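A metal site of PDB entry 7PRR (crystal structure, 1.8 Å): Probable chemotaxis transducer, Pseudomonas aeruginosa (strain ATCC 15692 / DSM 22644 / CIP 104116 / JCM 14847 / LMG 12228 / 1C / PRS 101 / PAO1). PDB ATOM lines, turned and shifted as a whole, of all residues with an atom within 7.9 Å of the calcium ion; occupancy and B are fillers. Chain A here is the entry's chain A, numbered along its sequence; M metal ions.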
ATOM      1  N   LEU A 275     -18.000 -32.159  -8.955  1.00  0.00           N
ATOM      2  CA  LEU A 275     -17.125 -31.470  -8.028  1.00  0.00           C
ATOM      3  C   LEU A 275     -16.892 -32.257  -6.736  1.00  0.00           C
ATOM      4  O   LEU A 275     -17.435 -33.346  -6.535  1.00  0.00           O
ATOM      5  CB  LEU A 275     -17.711 -30.089  -7.710  1.00  0.00           C
ATOM      6  CG  LEU A 275     -17.992 -29.225  -8.938  1.00  0.00           C
ATOM      7  CD1 LEU A 275     -18.277 -27.780  -8.553  1.00  0.00           C
ATOM      8  CD2 LEU A 275     -16.781 -29.266  -9.858  1.00  0.00           C
ATOM      9  N   ASP A 276     -16.054 -31.653  -5.876  1.00  0.00           N
ATOM     10  CA  ASP A 276     -15.563 -32.225  -4.628  1.00  0.00           C
ATOM     11  C   ASP A 276     -16.604 -32.130  -3.524  1.00  0.00           C
ATOM     12  O   ASP A 276     -17.463 -31.252  -3.539  1.00  0.00           O
ATOM     13  CB  ASP A 276     -14.324 -31.438  -4.180  1.00  0.00           C
ATOM     14  CG  ASP A 276     -13.129 -31.685  -5.060  1.00  0.00           C
ATOM     15  OD1 ASP A 276     -13.148 -32.663  -5.831  1.00  0.00           O
ATOM     16  OD2 ASP A 276     -12.174 -30.869  -5.007  1.00  0.00           O
ATOM     17  N   GLY A 277     -16.499 -33.016  -2.554  1.00  0.00           N
ATOM     18  CA  GLY A 277     -17.266 -32.824  -1.333  1.00  0.00           C
ATOM     19  C   GLY A 277     -17.045 -31.431  -0.769  1.00  0.00           C
ATOM     20  O   GLY A 277     -17.993 -30.701  -0.493  1.00  0.00           O
ATOM     21  N   ASN A 278     -15.776 -31.046  -0.630  1.00  0.00           N
ATOM     22  CA  ASN A 278     -15.439 -29.726  -0.140  1.00  0.00           C
ATOM     23  C   ASN A 278     -16.000 -28.639  -1.041  1.00  0.00           C
ATOM     24  O   ASN A 278     -16.544 -27.638  -0.554  1.00  0.00           O
ATOM     25  CB  ASN A 278     -13.912 -29.606  -0.024  1.00  0.00           C
ATOM     26  CG  ASN A 278     -13.478 -28.310   0.605  1.00  0.00           C
ATOM     27  OD1 ASN A 278     -13.747 -28.046   1.778  1.00  0.00           O
ATOM     28  ND2 ASN A 278     -12.801 -27.470  -0.191  1.00  0.00           N
ATOM     29  N   GLU A 279     -15.897 -28.821  -2.366  1.00  0.00           N
ATOM     30  CA  GLU A 279     -16.457 -27.838  -3.293  1.00  0.00           C
ATOM     31  C   GLU A 279     -17.982 -27.801  -3.219  1.00  0.00           C
ATOM     32  O   GLU A 279     -18.590 -26.720  -3.243  1.00  0.00           O
ATOM     33  CB  GLU A 279     -16.005 -28.139  -4.721  1.00  0.00           C
ATOM     34  CG  GLU A 279     -14.871 -27.240  -5.214  1.00  0.00           C
ATOM     35  CD  GLU A 279     -13.913 -27.951  -6.157  1.00  0.00           C
ATOM     36  OE1 GLU A 279     -14.260 -29.023  -6.692  1.00  0.00           O
ATOM     37  OE2 GLU A 279     -12.799 -27.417  -6.368  1.00  0.00           O
ATOM     38  N   VAL A 280     -18.621 -28.973  -3.139  1.00  0.00           N
ATOM     39  CA  VAL A 280     -20.080 -29.031  -3.080  1.00  0.00           C
ATOM     40  C   VAL A 280     -20.584 -28.394  -1.784  1.00  0.00           C
ATOM     41  O   VAL A 280     -21.637 -27.741  -1.785  1.00  0.00           O
ATOM     42  CB  VAL A 280     -20.562 -30.487  -3.221  1.00  0.00           C
ATOM     43  CG1 VAL A 280     -22.096 -30.561  -3.117  1.00  0.00           C
ATOM     44  CG2 VAL A 280     -20.113 -31.083  -4.535  1.00  0.00           C
ATOM     45  N   ASN A 282     -18.929 -25.934  -0.115  1.00  0.00           N
ATOM     46  CA  ASN A 282     -18.757 -24.508  -0.326  1.00  0.00           C
ATOM     47  C   ASN A 282     -19.846 -23.940  -1.225  1.00  0.00           C
ATOM     48  O   ASN A 282     -20.262 -22.790  -1.052  1.00  0.00           O
ATOM     49  CB  ASN A 282     -17.368 -24.227  -0.913  1.00  0.00           C
ATOM     50  CG  ASN A 282     -16.260 -24.348   0.119  1.00  0.00           C
ATOM     51  OD1 ASN A 282     -16.368 -23.840   1.256  1.00  0.00           O
ATOM     52  ND2 ASN A 282     -15.177 -25.021  -0.256  1.00  0.00           N
ATOM     53  N   ASP A 294     -11.497 -20.676  -0.638  1.00  0.00           N
ATOM     54  CA  ASP A 294     -11.160 -21.891   0.090  1.00  0.00           C
ATOM     55  C   ASP A 294      -9.904 -22.532  -0.489  1.00  0.00           C
ATOM     56  O   ASP A 294      -9.609 -22.392  -1.675  1.00  0.00           O
ATOM     57  CB  ASP A 294     -12.307 -22.918   0.071  1.00  0.00           C
ATOM     58  CG  ASP A 294     -12.336 -23.794   1.314  1.00  0.00           C
ATOM     59  OD1 ASP A 294     -11.368 -23.751   2.107  1.00  0.00           O
ATOM     60  OD2 ASP A 294     -13.328 -24.523   1.510  1.00  0.00           O
ATOM     61  N   ILE A 295      -9.176 -23.236   0.366  1.00  0.00           N
ATOM     62  CA  ILE A 295      -7.953 -23.931   0.000  1.00  0.00           C
ATOM     63  C   ILE A 295      -8.191 -25.420   0.204  1.00  0.00           C
ATOM     64  O   ILE A 295      -8.275 -25.887   1.345  1.00  0.00           O
ATOM     65  CB  ILE A 295      -6.740 -23.464   0.835  1.00  0.00           C
ATOM     66  CG1 ILE A 295      -6.605 -21.931   0.755  1.00  0.00           C
ATOM     67  CG2 ILE A 295      -5.482 -24.186   0.355  1.00  0.00           C
ATOM     68  CD1 ILE A 295      -5.771 -21.328   1.880  1.00  0.00           C
ATOM     69  N   ASP A 296      -8.295 -26.163  -0.892  1.00  0.00           N
ATOM     70  CA  ASP A 296      -8.388 -27.618  -0.831  1.00  0.00           C
ATOM     71  C   ASP A 296      -6.985 -28.197  -0.725  1.00  0.00           C
ATOM     72  O   ASP A 296      -6.315 -28.385  -1.736  1.00  0.00           O
ATOM     73  CB  ASP A 296      -9.124 -28.171  -2.053  1.00  0.00           C
ATOM     74  CG  ASP A 296      -9.895 -29.429  -1.736  1.00  0.00           C
ATOM     75  OD1 ASP A 296      -9.271 -30.387  -1.221  1.00  0.00           O
ATOM     76  OD2 ASP A 296     -11.108 -29.480  -2.020  1.00  0.00           O
ATOM     77  N   ALA A 297      -6.545 -28.455   0.508  1.00  0.00           N
ATOM     78  CA  ALA A 297      -5.199 -28.992   0.703  1.00  0.00           C
ATOM     79  C   ALA A 297      -5.065 -30.401   0.132  1.00  0.00           C
ATOM     80  O   ALA A 297      -3.983 -30.782  -0.325  1.00  0.00           O
ATOM     81  CB  ALA A 297      -4.844 -29.001   2.189  1.00  0.00           C
ATOM     82  N   GLU A 298      -6.140 -31.191   0.179  1.00  0.00           N
ATOM     83  CA  GLU A 298      -6.111 -32.551  -0.363  1.00  0.00           C
ATOM     84  C   GLU A 298      -5.642 -32.556  -1.816  1.00  0.00           C
ATOM     85  O   GLU A 298      -4.948 -33.496  -2.239  1.00  0.00           O
ATOM     86  CB  GLU A 298      -7.489 -33.195  -0.260  1.00  0.00           C
ATOM     87  CG  GLU A 298      -7.847 -33.675   1.136  1.00  0.00           C
ATOM     88  CD  GLU A 298      -8.742 -34.916   1.113  1.00  0.00           C
ATOM     89  OE1 GLU A 298      -9.963 -34.760   0.861  1.00  0.00           O
ATOM     90  OE2 GLU A 298      -8.217 -36.032   1.344  1.00  0.00           O
ATOM     91  N   HIS A 299      -5.997 -31.527  -2.579  1.00  0.00           N
ATOM     92  CA  HIS A 299      -5.654 -31.439  -3.988  1.00  0.00           C
ATOM     93  C   HIS A 299      -4.727 -30.274  -4.285  1.00  0.00           C
ATOM     94  O   HIS A 299      -4.373 -30.066  -5.453  1.00  0.00           O
ATOM     95  CB  HIS A 299      -6.931 -31.309  -4.830  1.00  0.00           C
ATOM     96  CG  HIS A 299      -7.939 -32.390  -4.554  1.00  0.00           C
ATOM     97  ND1 HIS A 299      -8.774 -32.360  -3.460  1.00  0.00           N
ATOM     98  CD2 HIS A 299      -8.231 -33.532  -5.218  1.00  0.00           C
ATOM     99  CE1 HIS A 299      -9.541 -33.440  -3.460  1.00  0.00           C
ATOM    100  NE2 HIS A 299      -9.227 -34.162  -4.523  1.00  0.00           N
ATOM    101  N   GLY A 300      -4.318 -29.508  -3.277  1.00  0.00           N
ATOM    102  CA  GLY A 300      -3.396 -28.403  -3.496  1.00  0.00           C
ATOM    103  C   GLY A 300      -3.884 -27.351  -4.481  1.00  0.00           C
ATOM    104  O   GLY A 300      -3.096 -26.869  -5.300  1.00  0.00           O
ATOM    105  N   HIS A 301      -5.154 -26.996  -4.436  1.00  0.00           N
ATOM    106  CA  HIS A 301      -5.557 -25.855  -5.233  1.00  0.00           C
ATOM    107  C   HIS A 301      -6.517 -24.968  -4.460  1.00  0.00           C
ATOM    108  O   HIS A 301      -7.081 -25.361  -3.444  1.00  0.00           O
ATOM    109  CB  HIS A 301      -6.162 -26.205  -6.606  1.00  0.00           C
ATOM    110  CG  HIS A 301      -7.063 -27.396  -6.609  1.00  0.00           C
ATOM    111  ND1 HIS A 301      -8.144 -27.521  -5.762  1.00  0.00           N
ATOM    112  CD2 HIS A 301      -7.067 -28.504  -7.398  1.00  0.00           C
ATOM    113  CE1 HIS A 301      -8.764 -28.667  -6.016  1.00  0.00           C
ATOM    114  NE2 HIS A 301      -8.133 -29.273  -6.998  1.00  0.00           N
ATOM    115  N   ILE A 302      -6.675 -23.772  -4.971  1.00  0.00           N
ATOM    116  CA  ILE A 302      -7.511 -22.744  -4.393  1.00  0.00           C
ATOM    117  C   ILE A 302      -8.856 -22.808  -5.074  1.00  0.00           C
ATOM    118  O   ILE A 302      -8.937 -23.035  -6.295  1.00  0.00           O
ATOM    119  CB  ILE A 302      -6.857 -21.356  -4.575  1.00  0.00           C
ATOM    120  CG1 ILE A 302      -5.470 -21.372  -3.933  1.00  0.00           C
ATOM    121  CG2 ILE A 302      -7.731 -20.266  -3.989  1.00  0.00           C
ATOM    122  CD1 ILE A 302      -4.662 -20.175  -4.258  1.00  0.00           C
ATOM    123  N   GLU A 303      -9.914 -22.648  -4.295  1.00  0.00           N
ATOM    124  CA  GLU A 303     -11.275 -22.592  -4.791  1.00  0.00           C
ATOM    125  C   GLU A 303     -11.796 -21.198  -4.547  1.00  0.00           C
ATOM    126  O   GLU A 303     -11.612 -20.644  -3.464  1.00  0.00           O
ATOM    127  CB  GLU A 303     -12.200 -23.604  -4.104  1.00  0.00           C
ATOM    128  CG  GLU A 303     -11.796 -25.055  -4.265  1.00  0.00           C
ATOM    129  CD  GLU A 303     -12.438 -25.935  -3.204  1.00  0.00           C
ATOM    130  OE1 GLU A 303     -13.364 -25.440  -2.510  1.00  0.00           O
ATOM    131  OE2 GLU A 303     -12.018 -27.101  -3.062  1.00  0.00           O
ATOM    132  N   PHE A 305     -15.460 -19.101  -5.345  1.00  0.00           N
ATOM    133  CA  PHE A 305     -16.830 -19.086  -5.846  1.00  0.00           C
ATOM    134  C   PHE A 305     -17.351 -17.657  -5.815  1.00  0.00           C
ATOM    135  O   PHE A 305     -17.338 -17.006  -4.768  1.00  0.00           O
ATOM    136  CB  PHE A 305     -17.740 -19.964  -5.005  1.00  0.00           C
ATOM    137  CG  PHE A 305     -17.317 -21.404  -4.961  1.00  0.00           C
ATOM    138  CD1 PHE A 305     -16.371 -21.823  -4.047  1.00  0.00           C
ATOM    139  CD2 PHE A 305     -17.873 -22.333  -5.818  1.00  0.00           C
ATOM    140  CE1 PHE A 305     -15.994 -23.153  -3.986  1.00  0.00           C
ATOM    141  CE2 PHE A 305     -17.490 -23.667  -5.769  1.00  0.00           C
ATOM    142  CZ  PHE A 305     -16.554 -24.060  -4.853  1.00  0.00           C
ATOM    143  N   MET A 320     -17.020 -20.549 -10.622  1.00  0.00           N
ATOM    144  CA  MET A 320     -16.061 -21.239  -9.779  1.00  0.00           C
ATOM    145  C   MET A 320     -14.709 -21.194 -10.465  1.00  0.00           C
ATOM    146  O   MET A 320     -14.607 -21.543 -11.642  1.00  0.00           O
ATOM    147  CB  MET A 320     -16.436 -22.692  -9.512  1.00  0.00           C
ATOM    148  CG  MET A 320     -15.507 -23.321  -8.474  1.00  0.00           C
ATOM    149  SD  MET A 320     -15.561 -25.137  -8.486  1.00  0.00           S
ATOM    150  CE  MET A 320     -14.534 -25.437  -9.940  1.00  0.00           C
ATOM    151  N   LEU A 321     -13.694 -20.743  -9.734  1.00  0.00           N
ATOM    152  CA  LEU A 321     -12.296 -20.800 -10.176  1.00  0.00           C
ATOM    153  C   LEU A 321     -11.603 -21.864  -9.329  1.00  0.00           C
ATOM    154  O   LEU A 321     -11.731 -21.845  -8.101  1.00  0.00           O
ATOM    155  CB  LEU A 321     -11.617 -19.449  -9.934  1.00  0.00           C
ATOM    156  CG  LEU A 321     -11.572 -18.471 -11.126  1.00  0.00           C
ATOM    157  CD1 LEU A 321     -12.981 -17.891 -11.293  1.00  0.00           C
ATOM    158  CD2 LEU A 321     -10.583 -17.369 -10.829  1.00  0.00           C
ATOM    159  N   GLN A 322     -10.888 -22.782  -9.991  1.00  0.00           N
ATOM    160  CA  GLN A 322     -10.062 -23.785  -9.337  1.00  0.00           C
ATOM    161  C   GLN A 322      -8.650 -23.663  -9.901  1.00  0.00           C
ATOM    162  O   GLN A 322      -8.410 -24.030 -11.047  1.00  0.00           O
ATOM    163  CB  GLN A 322     -10.630 -25.186  -9.549  1.00  0.00           C
ATOM    164  CG  GLN A 322      -9.958 -26.254  -8.768  1.00  0.00           C
ATOM    165  CD  GLN A 322     -10.412 -27.637  -9.207  1.00  0.00           C
ATOM    166  OE1 GLN A 322     -10.018 -28.117 -10.269  1.00  0.00           O
ATOM    167  NE2 GLN A 322     -11.260 -28.263  -8.402  1.00  0.00           N
HETATM  168 CA    CA M   1     -11.221 -28.667  -4.444  1.00  0.00          CA
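A ring nitrogen (ND1) of His 299 sits at hydrogen-bond distance from the side-chain carboxylate (OD1) of Asp 296 (3.0 Å).
The side-chain amide nitrogen (ND2) of Asn 278 sits at hydrogen-bond distance from the side-chain carboxylate (OE1) of Glu 303 (3.1 Å).
The side-chain carboxylate (OE2) of Glu 279 lies close to the side-chain amide nitrogen (NE2) of Gln 322 (2.7 Å).
OE1 of Glu 303 lies within hydrogen-bond range of ND2 of Asn 282 (2.9 Å).
The backbone NH of Asp 296 lies within hydrogen-bond range of the backbone carbonyl oxygen of His 301.
The backbone NH (N) of Glu 303 lies within hydrogen-bond range of the backbone carbonyl oxygen (O) of Asp 294, at 2.7 Å.
The side-chain amide nitrogen (ND2) of Asn 278 lies close to the side-chain carboxylate (OD2) of Asp 296.
The calcium ion is bound by the side-chain carboxylate of Glu 303 (2.2 Å), the side-chain carboxylate of Asp 276 (2.5 Å), the side-chain carboxylate of Asp 296 (2.6 Å) and the side-chain carboxylate of Glu 279 (2.8 Å).
His 301 touches the calcium ion (CE1 to CA, 2.9 Å).
NE2 of Gln 322 touches the calcium ion (3.98 Å).
Of the 21 residues printed, 6 come within 4 Å of the calcium ion.
Along chain A the residues within 4 Å of the calcium ion span positions 276 to 322.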
